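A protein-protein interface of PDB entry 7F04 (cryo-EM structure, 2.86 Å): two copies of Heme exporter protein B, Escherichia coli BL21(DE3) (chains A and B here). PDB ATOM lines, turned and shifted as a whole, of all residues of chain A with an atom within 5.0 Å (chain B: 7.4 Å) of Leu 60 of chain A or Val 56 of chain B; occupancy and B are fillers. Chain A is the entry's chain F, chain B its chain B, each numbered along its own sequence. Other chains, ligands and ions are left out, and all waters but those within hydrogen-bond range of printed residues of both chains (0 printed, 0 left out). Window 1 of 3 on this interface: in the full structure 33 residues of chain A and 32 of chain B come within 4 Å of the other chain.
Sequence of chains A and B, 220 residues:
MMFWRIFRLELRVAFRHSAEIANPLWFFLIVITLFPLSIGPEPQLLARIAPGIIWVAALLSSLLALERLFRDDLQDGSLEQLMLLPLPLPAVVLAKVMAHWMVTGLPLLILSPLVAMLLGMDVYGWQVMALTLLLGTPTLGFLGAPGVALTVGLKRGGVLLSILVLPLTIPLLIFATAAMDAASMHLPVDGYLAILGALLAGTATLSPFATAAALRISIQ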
ATOM      1  N   PHE A  27     -22.116  -7.046  34.727  1.00  0.00           N
ATOM      2  CA  PHE A  27     -21.742  -7.636  33.448  1.00  0.00           C
ATOM      3  C   PHE A  27     -21.570  -9.143  33.566  1.00  0.00           C
ATOM      4  O   PHE A  27     -22.006  -9.895  32.690  1.00  0.00           O
ATOM      5  CB  PHE A  27     -20.461  -6.995  32.926  1.00  0.00           C
ATOM      6  CG  PHE A  27     -20.095  -7.422  31.536  1.00  0.00           C
ATOM      7  CD1 PHE A  27     -20.794  -6.944  30.445  1.00  0.00           C
ATOM      8  CD2 PHE A  27     -19.056  -8.307  31.321  1.00  0.00           C
ATOM      9  CE1 PHE A  27     -20.460  -7.335  29.169  1.00  0.00           C
ATOM     10  CE2 PHE A  27     -18.722  -8.701  30.047  1.00  0.00           C
ATOM     11  CZ  PHE A  27     -19.424  -8.216  28.970  1.00  0.00           C
ATOM     12  N   VAL A  31     -23.831 -11.796  31.503  1.00  0.00           N
ATOM     13  CA  VAL A  31     -23.203 -12.744  30.591  1.00  0.00           C
ATOM     14  C   VAL A  31     -23.573 -14.174  30.962  1.00  0.00           C
ATOM     15  O   VAL A  31     -23.905 -14.985  30.091  1.00  0.00           O
ATOM     16  CB  VAL A  31     -21.679 -12.539  30.558  1.00  0.00           C
ATOM     17  CG1 VAL A  31     -21.022 -13.651  29.765  1.00  0.00           C
ATOM     18  CG2 VAL A  31     -21.347 -11.200  29.939  1.00  0.00           C
ATOM     19  N   LEU A  34     -27.462 -14.615  30.005  1.00  0.00           N
ATOM     20  CA  LEU A  34     -27.938 -14.474  28.632  1.00  0.00           C
ATOM     21  C   LEU A  34     -27.942 -15.809  27.897  1.00  0.00           C
ATOM     22  O   LEU A  34     -28.905 -16.140  27.198  1.00  0.00           O
ATOM     23  CB  LEU A  34     -27.072 -13.457  27.890  1.00  0.00           C
ATOM     24  CG  LEU A  34     -27.529 -13.012  26.501  1.00  0.00           C
ATOM     25  CD1 LEU A  34     -28.804 -12.189  26.586  1.00  0.00           C
ATOM     26  CD2 LEU A  34     -26.425 -12.225  25.817  1.00  0.00           C
ATOM     27  N   PHE A  35     -26.862 -16.580  28.026  1.00  0.00           N
ATOM     28  CA  PHE A  35     -26.778 -17.857  27.319  1.00  0.00           C
ATOM     29  C   PHE A  35     -27.825 -18.866  27.777  1.00  0.00           C
ATOM     30  O   PHE A  35     -28.455 -19.499  26.912  1.00  0.00           O
ATOM     31  CB  PHE A  35     -25.358 -18.418  27.439  1.00  0.00           C
ATOM     32  CG  PHE A  35     -24.317 -17.587  26.748  1.00  0.00           C
ATOM     33  CD1 PHE A  35     -23.709 -16.533  27.400  1.00  0.00           C
ATOM     34  CD2 PHE A  35     -23.940 -17.870  25.450  1.00  0.00           C
ATOM     35  CE1 PHE A  35     -22.751 -15.771  26.768  1.00  0.00           C
ATOM     36  CE2 PHE A  35     -22.981 -17.114  24.815  1.00  0.00           C
ATOM     37  CZ  PHE A  35     -22.385 -16.064  25.474  1.00  0.00           C
ATOM     38  N   VAL A  56     -15.376 -17.159  30.648  1.00  0.00           N
ATOM     39  CA  VAL A  56     -15.330 -16.006  29.756  1.00  0.00           C
ATOM     40  C   VAL A  56     -15.931 -14.786  30.441  1.00  0.00           C
ATOM     41  O   VAL A  56     -15.410 -13.670  30.323  1.00  0.00           O
ATOM     42  CB  VAL A  56     -16.039 -16.325  28.426  1.00  0.00           C
ATOM     43  CG1 VAL A  56     -16.306 -15.053  27.648  1.00  0.00           C
ATOM     44  CG2 VAL A  56     -15.197 -17.274  27.597  1.00  0.00           C
ATOM     45  N   ALA A  57     -17.032 -14.977  31.171  1.00  0.00           N
ATOM     46  CA  ALA A  57     -17.625 -13.882  31.929  1.00  0.00           C
ATOM     47  C   ALA A  57     -16.670 -13.376  32.997  1.00  0.00           C
ATOM     48  O   ALA A  57     -16.557 -12.166  33.212  1.00  0.00           O
ATOM     49  CB  ALA A  57     -18.939 -14.334  32.560  1.00  0.00           C
ATOM     50  N   ALA A  58     -15.979 -14.289  33.682  1.00  0.00           N
ATOM     51  CA  ALA A  58     -14.989 -13.871  34.670  1.00  0.00           C
ATOM     52  C   ALA A  58     -13.880 -13.048  34.026  1.00  0.00           C
ATOM     53  O   ALA A  58     -13.493 -11.997  34.549  1.00  0.00           O
ATOM     54  CB  ALA A  58     -14.409 -15.093  35.381  1.00  0.00           C
ATOM     55  N   LEU A  59     -13.373 -13.501  32.878  1.00  0.00           N
ATOM     56  CA  LEU A  59     -12.321 -12.764  32.183  1.00  0.00           C
ATOM     57  C   LEU A  59     -12.793 -11.373  31.778  1.00  0.00           C
ATOM     58  O   LEU A  59     -12.095 -10.377  31.998  1.00  0.00           O
ATOM     59  CB  LEU A  59     -11.865 -13.545  30.952  1.00  0.00           C
ATOM     60  CG  LEU A  59     -10.556 -14.326  31.027  1.00  0.00           C
ATOM     61  CD1 LEU A  59     -10.636 -15.416  32.079  1.00  0.00           C
ATOM     62  CD2 LEU A  59     -10.232 -14.916  29.668  1.00  0.00           C
ATOM     63  N   LEU A  60     -13.981 -11.286  31.182  1.00  0.00           N
ATOM     64  CA  LEU A  60     -14.464 -10.003  30.685  1.00  0.00           C
ATOM     65  C   LEU A  60     -14.792  -9.051  31.828  1.00  0.00           C
ATOM     66  O   LEU A  60     -14.556  -7.843  31.724  1.00  0.00           O
ATOM     67  CB  LEU A  60     -15.677 -10.219  29.785  1.00  0.00           C
ATOM     68  CG  LEU A  60     -15.429 -11.030  28.511  1.00  0.00           C
ATOM     69  CD1 LEU A  60     -16.586 -10.873  27.543  1.00  0.00           C
ATOM     70  CD2 LEU A  60     -14.123 -10.623  27.856  1.00  0.00           C
ATOM     71  N   SER A  61     -15.331  -9.575  32.931  1.00  0.00           N
ATOM     72  CA  SER A  61     -15.550  -8.751  34.112  1.00  0.00           C
ATOM     73  C   SER A  61     -14.232  -8.241  34.677  1.00  0.00           C
ATOM     74  O   SER A  61     -14.141  -7.090  35.124  1.00  0.00           O
ATOM     75  CB  SER A  61     -16.318  -9.552  35.163  1.00  0.00           C
ATOM     76  OG  SER A  61     -16.217  -8.951  36.440  1.00  0.00           O
ATOM     77  N   SER A  62     -13.197  -9.086  34.672  1.00  0.00           N
ATOM     78  CA  SER A  62     -11.885  -8.644  35.132  1.00  0.00           C
ATOM     79  C   SER A  62     -11.337  -7.528  34.254  1.00  0.00           C
ATOM     80  O   SER A  62     -10.761  -6.561  34.759  1.00  0.00           O
ATOM     81  CB  SER A  62     -10.920  -9.827  35.167  1.00  0.00           C
ATOM     82  OG  SER A  62     -11.248 -10.715  36.221  1.00  0.00           O
ATOM     83  N   LEU A  63     -11.497  -7.648  32.935  1.00  0.00           N
ATOM     84  CA  LEU A  63     -11.082  -6.565  32.042  1.00  0.00           C
ATOM     85  C   LEU A  63     -11.880  -5.291  32.284  1.00  0.00           C
ATOM     86  O   LEU A  63     -11.330  -4.187  32.211  1.00  0.00           O
ATOM     87  CB  LEU A  63     -11.183  -6.994  30.578  1.00  0.00           C
ATOM     88  CG  LEU A  63     -10.011  -7.775  29.977  1.00  0.00           C
ATOM     89  CD1 LEU A  63      -8.804  -6.867  29.982  1.00  0.00           C
ATOM     90  CD2 LEU A  63      -9.683  -9.047  30.728  1.00  0.00           C
ATOM     91  N   LEU A  64     -13.180  -5.417  32.554  1.00  0.00           N
ATOM     92  CA  LEU A  64     -13.974  -4.231  32.864  1.00  0.00           C
ATOM     93  C   LEU A  64     -13.481  -3.554  34.136  1.00  0.00           C
ATOM     94  O   LEU A  64     -13.418  -2.322  34.209  1.00  0.00           O
ATOM     95  CB  LEU A  64     -15.449  -4.600  33.000  1.00  0.00           C
ATOM     96  CG  LEU A  64     -16.326  -4.339  31.779  1.00  0.00           C
ATOM     97  CD1 LEU A  64     -17.755  -4.736  32.076  1.00  0.00           C
ATOM     98  CD2 LEU A  64     -16.246  -2.882  31.366  1.00  0.00           C
ATOM     99  N   LEU A 166      -5.491  -9.620  27.263  1.00  0.00           N
ATOM    100  CA  LEU A 166      -6.470 -10.661  26.986  1.00  0.00           C
ATOM    101  C   LEU A 166      -5.825 -11.881  26.332  1.00  0.00           C
ATOM    102  O   LEU A 166      -6.194 -13.012  26.668  1.00  0.00           O
ATOM    103  CB  LEU A 166      -7.607 -10.112  26.124  1.00  0.00           C
ATOM    104  CG  LEU A 166      -8.958 -10.813  26.245  1.00  0.00           C
ATOM    105  CD1 LEU A 166      -9.381 -10.886  27.694  1.00  0.00           C
ATOM    106  CD2 LEU A 166     -10.007 -10.075  25.435  1.00  0.00           C
ATOM    107  N   PHE B  27      -9.878  -5.968  18.820  1.00  0.00           N
ATOM    108  CA  PHE B  27     -10.555  -6.274  20.076  1.00  0.00           C
ATOM    109  C   PHE B  27     -11.698  -7.255  19.854  1.00  0.00           C
ATOM    110  O   PHE B  27     -11.849  -8.237  20.593  1.00  0.00           O
ATOM    111  CB  PHE B  27     -11.068  -4.984  20.716  1.00  0.00           C
ATOM    112  CG  PHE B  27     -12.173  -5.195  21.713  1.00  0.00           C
ATOM    113  CD1 PHE B  27     -11.889  -5.597  23.005  1.00  0.00           C
ATOM    114  CD2 PHE B  27     -13.494  -4.979  21.363  1.00  0.00           C
ATOM    115  CE1 PHE B  27     -12.899  -5.786  23.924  1.00  0.00           C
ATOM    116  CE2 PHE B  27     -14.508  -5.171  22.277  1.00  0.00           C
ATOM    117  CZ  PHE B  27     -14.210  -5.573  23.558  1.00  0.00           C
ATOM    118  N   PHE B  28     -12.516  -7.003  18.831  1.00  0.00           N
ATOM    119  CA  PHE B  28     -13.623  -7.904  18.530  1.00  0.00           C
ATOM    120  C   PHE B  28     -13.114  -9.281  18.136  1.00  0.00           C
ATOM    121  O   PHE B  28     -13.690 -10.299  18.532  1.00  0.00           O
ATOM    122  CB  PHE B  28     -14.498  -7.313  17.427  1.00  0.00           C
ATOM    123  CG  PHE B  28     -15.426  -6.237  17.906  1.00  0.00           C
ATOM    124  CD1 PHE B  28     -16.272  -6.461  18.975  1.00  0.00           C
ATOM    125  CD2 PHE B  28     -15.449  -5.000  17.291  1.00  0.00           C
ATOM    126  CE1 PHE B  28     -17.125  -5.473  19.419  1.00  0.00           C
ATOM    127  CE2 PHE B  28     -16.297  -4.007  17.733  1.00  0.00           C
ATOM    128  CZ  PHE B  28     -17.138  -4.245  18.798  1.00  0.00           C
ATOM    129  N   ILE B  30     -10.307 -10.750  19.104  1.00  0.00           N
ATOM    130  CA  ILE B  30      -9.818 -11.437  20.297  1.00  0.00           C
ATOM    131  C   ILE B  30     -10.980 -11.929  21.152  1.00  0.00           C
ATOM    132  O   ILE B  30     -10.962 -13.057  21.664  1.00  0.00           O
ATOM    133  CB  ILE B  30      -8.877 -10.517  21.096  1.00  0.00           C
ATOM    134  CG1 ILE B  30      -7.648 -10.158  20.263  1.00  0.00           C
ATOM    135  CG2 ILE B  30      -8.441 -11.191  22.380  1.00  0.00           C
ATOM    136  CD1 ILE B  30      -6.706  -9.208  20.950  1.00  0.00           C
ATOM    137  N   VAL B  31     -12.008 -11.093  21.324  1.00  0.00           N
ATOM    138  CA  VAL B  31     -13.160 -11.503  22.122  1.00  0.00           C
ATOM    139  C   VAL B  31     -13.859 -12.695  21.479  1.00  0.00           C
ATOM    140  O   VAL B  31     -14.285 -13.628  22.170  1.00  0.00           O
ATOM    141  CB  VAL B  31     -14.120 -10.318  22.327  1.00  0.00           C
ATOM    142  CG1 VAL B  31     -15.407 -10.786  22.977  1.00  0.00           C
ATOM    143  CG2 VAL B  31     -13.461  -9.258  23.181  1.00  0.00           C
ATOM    144  N   LEU B  34     -11.906 -15.830  22.117  1.00  0.00           N
ATOM    145  CA  LEU B  34     -11.936 -16.301  23.501  1.00  0.00           C
ATOM    146  C   LEU B  34     -12.925 -17.445  23.710  1.00  0.00           C
ATOM    147  O   LEU B  34     -12.748 -18.250  24.628  1.00  0.00           O
ATOM    148  CB  LEU B  34     -12.283 -15.148  24.440  1.00  0.00           C
ATOM    149  CG  LEU B  34     -11.137 -14.269  24.934  1.00  0.00           C
ATOM    150  CD1 LEU B  34     -11.624 -13.385  26.062  1.00  0.00           C
ATOM    151  CD2 LEU B  34      -9.963 -15.115  25.383  1.00  0.00           C
ATOM    152  N   PHE B  35     -13.967 -17.530  22.889  1.00  0.00           N
ATOM    153  CA  PHE B  35     -15.053 -18.476  23.131  1.00  0.00           C
ATOM    154  C   PHE B  35     -14.746 -19.902  22.672  1.00  0.00           C
ATOM    155  O   PHE B  35     -15.071 -20.846  23.400  1.00  0.00           O
ATOM    156  CB  PHE B  35     -16.342 -17.975  22.480  1.00  0.00           C
ATOM    157  CG  PHE B  35     -17.077 -16.962  23.303  1.00  0.00           C
ATOM    158  CD1 PHE B  35     -16.708 -15.631  23.275  1.00  0.00           C
ATOM    159  CD2 PHE B  35     -18.128 -17.343  24.116  1.00  0.00           C
ATOM    160  CE1 PHE B  35     -17.381 -14.699  24.032  1.00  0.00           C
ATOM    161  CE2 PHE B  35     -18.803 -16.415  24.875  1.00  0.00           C
ATOM    162  CZ  PHE B  35     -18.431 -15.091  24.832  1.00  0.00           C
ATOM    163  N   ALA B  50     -23.521 -18.484  18.927  1.00  0.00           N
ATOM    164  CA  ALA B  50     -23.066 -17.263  18.264  1.00  0.00           C
ATOM    165  C   ALA B  50     -23.832 -15.997  18.636  1.00  0.00           C
ATOM    166  O   ALA B  50     -23.180 -14.951  18.795  1.00  0.00           O
ATOM    167  CB  ALA B  50     -23.092 -17.473  16.744  1.00  0.00           C
ATOM    168  N   PRO B  51     -25.170 -15.987  18.740  1.00  0.00           N
ATOM    169  CA  PRO B  51     -25.836 -14.737  19.150  1.00  0.00           C
ATOM    170  C   PRO B  51     -25.333 -14.203  20.475  1.00  0.00           C
ATOM    171  O   PRO B  51     -25.081 -12.995  20.608  1.00  0.00           O
ATOM    172  CB  PRO B  51     -27.315 -15.139  19.229  1.00  0.00           C
ATOM    173  CG  PRO B  51     -27.441 -16.305  18.342  1.00  0.00           C
ATOM    174  CD  PRO B  51     -26.148 -17.043  18.420  1.00  0.00           C
ATOM    175  N   GLY B  52     -25.156 -15.085  21.458  1.00  0.00           N
ATOM    176  CA  GLY B  52     -24.625 -14.657  22.737  1.00  0.00           C
ATOM    177  C   GLY B  52     -23.218 -14.110  22.624  1.00  0.00           C
ATOM    178  O   GLY B  52     -22.895 -13.090  23.226  1.00  0.00           O
ATOM    179  N   ILE B  53     -22.364 -14.776  21.843  1.00  0.00           N
ATOM    180  CA  ILE B  53     -20.993 -14.304  21.664  1.00  0.00           C
ATOM    181  C   ILE B  53     -20.992 -12.897  21.090  1.00  0.00           C
ATOM    182  O   ILE B  53     -20.338 -11.984  21.615  1.00  0.00           O
ATOM    183  CB  ILE B  53     -20.209 -15.266  20.755  1.00  0.00           C
ATOM    184  CG1 ILE B  53     -20.179 -16.671  21.339  1.00  0.00           C
ATOM    185  CG2 ILE B  53     -18.800 -14.770  20.552  1.00  0.00           C
ATOM    186  CD1 ILE B  53     -19.507 -17.671  20.431  1.00  0.00           C
ATOM    187  N   ILE B  54     -21.743 -12.700  20.007  1.00  0.00           N
ATOM    188  CA  ILE B  54     -21.738 -11.423  19.308  1.00  0.00           C
ATOM    189  C   ILE B  54     -22.275 -10.319  20.204  1.00  0.00           C
ATOM    190  O   ILE B  54     -21.695  -9.227  20.283  1.00  0.00           O
ATOM    191  CB  ILE B  54     -22.541 -11.542  18.003  1.00  0.00           C
ATOM    192  CG1 ILE B  54     -21.736 -12.328  16.973  1.00  0.00           C
ATOM    193  CG2 ILE B  54     -22.905 -10.170  17.468  1.00  0.00           C
ATOM    194  CD1 ILE B  54     -22.575 -13.192  16.082  1.00  0.00           C
ATOM    195  N   TRP B  55     -23.374 -10.579  20.910  1.00  0.00           N
ATOM    196  CA  TRP B  55     -23.968  -9.505  21.688  1.00  0.00           C
ATOM    197  C   TRP B  55     -23.232  -9.258  22.999  1.00  0.00           C
ATOM    198  O   TRP B  55     -23.233  -8.128  23.490  1.00  0.00           O
ATOM    199  CB  TRP B  55     -25.450  -9.785  21.901  1.00  0.00           C
ATOM    200  CG  TRP B  55     -26.218  -9.248  20.748  1.00  0.00           C
ATOM    201  CD1 TRP B  55     -26.828  -9.961  19.765  1.00  0.00           C
ATOM    202  CD2 TRP B  55     -26.401  -7.868  20.415  1.00  0.00           C
ATOM    203  NE1 TRP B  55     -27.403  -9.113  18.851  1.00  0.00           N
ATOM    204  CE2 TRP B  55     -27.151  -7.821  19.228  1.00  0.00           C
ATOM    205  CE3 TRP B  55     -26.013  -6.667  21.014  1.00  0.00           C
ATOM    206  CZ2 TRP B  55     -27.525  -6.623  18.632  1.00  0.00           C
ATOM    207  CZ3 TRP B  55     -26.382  -5.480  20.419  1.00  0.00           C
ATOM    208  CH2 TRP B  55     -27.132  -5.466  19.241  1.00  0.00           C
ATOM    209  N   VAL B  56     -22.560 -10.267  23.556  1.00  0.00           N
ATOM    210  CA  VAL B  56     -21.666 -10.019  24.681  1.00  0.00           C
ATOM    211  C   VAL B  56     -20.491  -9.153  24.245  1.00  0.00           C
ATOM    212  O   VAL B  56     -20.085  -8.236  24.965  1.00  0.00           O
ATOM    213  CB  VAL B  56     -21.200 -11.348  25.303  1.00  0.00           C
ATOM    214  CG1 VAL B  56     -20.043 -11.113  26.249  1.00  0.00           C
ATOM    215  CG2 VAL B  56     -22.344 -12.002  26.058  1.00  0.00           C
ATOM    216  N   ALA B  57     -19.930  -9.421  23.063  1.00  0.00           N
ATOM    217  CA  ALA B  57     -18.851  -8.574  22.563  1.00  0.00           C
ATOM    218  C   ALA B  57     -19.327  -7.144  22.339  1.00  0.00           C
ATOM    219  O   ALA B  57     -18.628  -6.183  22.688  1.00  0.00           O
ATOM    220  CB  ALA B  57     -18.280  -9.157  21.273  1.00  0.00           C
ATOM    221  N   ALA B  58     -20.519  -6.985  21.758  1.00  0.00           N
ATOM    222  CA  ALA B  58     -21.065  -5.649  21.534  1.00  0.00           C
ATOM    223  C   ALA B  58     -21.300  -4.916  22.849  1.00  0.00           C
ATOM    224  O   ALA B  58     -20.963  -3.733  22.978  1.00  0.00           O
ATOM    225  CB  ALA B  58     -22.364  -5.743  20.737  1.00  0.00           C
ATOM    226  N   LEU B  59     -21.875  -5.605  23.837  1.00  0.00           N
ATOM    227  CA  LEU B  59     -22.110  -4.993  25.139  1.00  0.00           C
ATOM    228  C   LEU B  59     -20.801  -4.606  25.811  1.00  0.00           C
ATOM    229  O   LEU B  59     -20.705  -3.538  26.421  1.00  0.00           O
ATOM    230  CB  LEU B  59     -22.905  -5.948  26.028  1.00  0.00           C
ATOM    231  CG  LEU B  59     -23.254  -5.455  27.430  1.00  0.00           C
ATOM    232  CD1 LEU B  59     -24.153  -4.235  27.362  1.00  0.00           C
ATOM    233  CD2 LEU B  59     -23.907  -6.561  28.237  1.00  0.00           C
ATOM    234  N   LEU B  60     -19.784  -5.464  25.717  1.00  0.00           N
ATOM    235  CA  LEU B  60     -18.495  -5.146  26.322  1.00  0.00           C
ATOM    236  C   LEU B  60     -17.867  -3.921  25.674  1.00  0.00           C
ATOM    237  O   LEU B  60     -17.349  -3.040  26.370  1.00  0.00           O
ATOM    238  CB  LEU B  60     -17.557  -6.348  26.218  1.00  0.00           C
ATOM    239  CG  LEU B  60     -16.172  -6.175  26.840  1.00  0.00           C
ATOM    240  CD1 LEU B  60     -16.277  -5.991  28.341  1.00  0.00           C
ATOM    241  CD2 LEU B  60     -15.292  -7.361  26.508  1.00  0.00           C
ATOM    242  N   SER B  61     -17.900  -3.844  24.340  1.00  0.00           N
ATOM    243  CA  SER B  61     -17.334  -2.681  23.664  1.00  0.00           C
ATOM    244  C   SER B  61     -18.090  -1.410  24.029  1.00  0.00           C
ATOM    245  O   SER B  61     -17.478  -0.361  24.277  1.00  0.00           O
ATOM    246  CB  SER B  61     -17.339  -2.894  22.152  1.00  0.00           C
ATOM    247  OG  SER B  61     -18.657  -2.871  21.637  1.00  0.00           O
ATOM    248  N   SER B  62     -19.423  -1.482  24.073  1.00  0.00           N
ATOM    249  CA  SER B  62     -20.214  -0.314  24.445  1.00  0.00           C
ATOM    250  C   SER B  62     -19.914   0.126  25.871  1.00  0.00           C
ATOM    251  O   SER B  62     -19.786   1.324  26.142  1.00  0.00           O
ATOM    252  CB  SER B  62     -21.702  -0.613  24.279  1.00  0.00           C
ATOM    253  OG  SER B  62     -22.031  -0.794  22.914  1.00  0.00           O
ATOM    254  N   LEU B  63     -19.800  -0.827  26.797  1.00  0.00           N
ATOM    255  CA  LEU B  63     -19.484  -0.488  28.179  1.00  0.00           C
ATOM    256  C   LEU B  63     -18.109   0.149  28.291  1.00  0.00           C
ATOM    257  O   LEU B  63     -17.926   1.121  29.033  1.00  0.00           O
ATOM    258  CB  LEU B  63     -19.550  -1.735  29.053  1.00  0.00           C
ATOM    259  CG  LEU B  63     -20.925  -2.296  29.391  1.00  0.00           C
ATOM    260  CD1 LEU B  63     -20.739  -3.488  30.294  1.00  0.00           C
ATOM    261  CD2 LEU B  63     -21.789  -1.239  30.051  1.00  0.00           C
ATOM    262  N   LEU B  64     -17.124  -0.397  27.576  1.00  0.00           N
ATOM    263  CA  LEU B  64     -15.784   0.173  27.624  1.00  0.00           C
ATOM    264  C   LEU B  64     -15.775   1.599  27.093  1.00  0.00           C
ATOM    265  O   LEU B  64     -15.172   2.491  27.700  1.00  0.00           O
ATOM    266  CB  LEU B  64     -14.811  -0.700  26.834  1.00  0.00           C
ATOM    267  CG  LEU B  64     -14.450  -2.047  27.460  1.00  0.00           C
ATOM    268  CD1 LEU B  64     -13.716  -2.918  26.458  1.00  0.00           C
ATOM    269  CD2 LEU B  64     -13.619  -1.853  28.716  1.00  0.00           C
ATOM    270  N   LEU B 108     -17.902  -3.575  14.629  1.00  0.00           N
ATOM    271  CA  LEU B 108     -18.557  -4.875  14.669  1.00  0.00           C
ATOM    272  C   LEU B 108     -19.401  -5.122  13.427  1.00  0.00           C
ATOM    273  O   LEU B 108     -19.533  -6.270  12.992  1.00  0.00           O
ATOM    274  CB  LEU B 108     -19.415  -4.996  15.928  1.00  0.00           C
ATOM    275  CG  LEU B 108     -19.887  -6.405  16.291  1.00  0.00           C
ATOM    276  CD1 LEU B 108     -18.797  -7.428  16.020  1.00  0.00           C
ATOM    277  CD2 LEU B 108     -20.308  -6.457  17.746  1.00  0.00           C
ATOM    278  N   LEU B 173     -30.697  -6.763  24.817  1.00  0.00           N
ATOM    279  CA  LEU B 173     -29.938  -7.995  24.633  1.00  0.00           C
ATOM    280  C   LEU B 173     -30.868  -9.172  24.387  1.00  0.00           C
ATOM    281  O   LEU B 173     -30.630  -9.984  23.486  1.00  0.00           O
ATOM    282  CB  LEU B 173     -29.069  -8.254  25.864  1.00  0.00           C
ATOM    283  CG  LEU B 173     -27.630  -7.731  25.924  1.00  0.00           C
ATOM    284  CD1 LEU B 173     -26.734  -8.520  24.996  1.00  0.00           C
ATOM    285  CD2 LEU B 173     -27.560  -6.249  25.600  1.00  0.00           C
ATOM    286  N   THR B 177     -30.749 -11.081  20.776  1.00  0.00           N
ATOM    287  CA  THR B 177     -30.347 -12.480  20.762  1.00  0.00           C
ATOM    288  C   THR B 177     -31.492 -13.385  20.335  1.00  0.00           C
ATOM    289  O   THR B 177     -31.258 -14.389  19.662  1.00  0.00           O
ATOM    290  CB  THR B 177     -29.822 -12.896  22.133  1.00  0.00           C
ATOM    291  OG1 THR B 177     -30.782 -12.553  23.138  1.00  0.00           O
ATOM    292  CG2 THR B 177     -28.511 -12.194  22.434  1.00  0.00           C
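Of the printed residues of chain B, Leu 60 of chain A touches Val 56 (3.7 Å) and Leu 60 (3.7 Å). Of the printed residues of chain A, Val 56 of chain B touches Val 31, Phe 35 and Leu 60. Of the printed residues of chain A, Thr 177 of chain B touches Leu 34 (3.97 Å). Printed residues of chain A within 4 Å of Leu 59 of chain B: Phe 27. Phe 27 of chain B touches none of the printed residues of chain A. Ala 58 of chain B touches none of the printed residues of chain A. The nearest printed residue of chain A that does not touch Leu 63 of chain B is Leu 60 of chain A (7.7 Å).
Of the 14 printed residues of chain A, 8 touch a printed residue of chain B. Hydrophobic or aromatic side chains of chain A that line the printed part of chain B: Phe 27, Val 31, Leu 34, Phe 35, Val 56, Leu 60, Leu 64 and Leu 166. Along chain A the printed residues that touch a printed residue of chain B span positions 27 to 166. Among the printed residues, no Asp or Glu carboxylate lies within 4 Å of a Lys or Arg side-chain nitrogen of the other chain.
The backbone carbonyl oxygen of Leu 173 of chain B sits at hydrogen-bond distance from the side-chain hydroxyl of Thr 177 of chain B (2.6 Å).
Phe 27 of chain A touches Leu 59 of chain B, but with the chains exchanged Leu 59 of chain A does not touch Phe 27 of chain B (9.3 Å). Phe 35 of chain A touches its own counterpart, Phe 35 of chain B. Phe 35 of chain A touches Val 56 of chain B, and with the chains exchanged Val 56 of chain A touches Phe 35 of chain B. Leu 64 of chain A touches Leu 60 of chain B, but with the chains exchanged Leu 60 of chain A does not touch Leu 64 of chain B (6.8 Å). Positions printed for both chains: 27, 31, 34, 35, 56, 57, 58, 59, 60, 61, 62, 63 and 64.
Among the printed residues, merely in contact across the chains: Phe 27 of chain A with Leu 63 of chain B (3.5 Å), Val 56 of chain A with Phe 35 of chain B (3.5 Å), Phe 35 of chain A with Gly 52 of chain B (3.6 Å), Leu 166 of chain A with Ile 30 of chain B (3.6 Å), Phe 35 of chain A with Phe 35 of chain B (3.6 Å), Phe 27 of chain A with Leu 59 of chain B (3.7 Å), Leu 64 of chain A with Leu 63 of chain B (3.7 Å), Leu 60 of chain A with Val 56 of chain B (3.7 Å), Leu 166 of chain A with Leu 34 of chain B (3.7 Å), Leu 60 of chain A with Leu 60 of chain B (3.7 Å), Leu 34 of chain A with Leu 173 of chain B (3.8 Å), Phe 27 of chain A with Leu 60 of chain B (3.8 Å), Leu 64 of chain A with Leu 60 of chain B (3.8 Å), Phe 35 of chain A with Ile 53 of chain B (3.8 Å), Phe 35 of chain A with Val 56 of chain B (3.9 Å), Leu 64 of chain A with Leu 64 of chain B (3.9 Å), Val 31 of chain A with Val 56 of chain B (3.9 Å), Val 56 of chain A with Leu 34 of chain B (3.97 Å) and Leu 34 of chain A with Thr 177 of chain B (3.97 Å).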
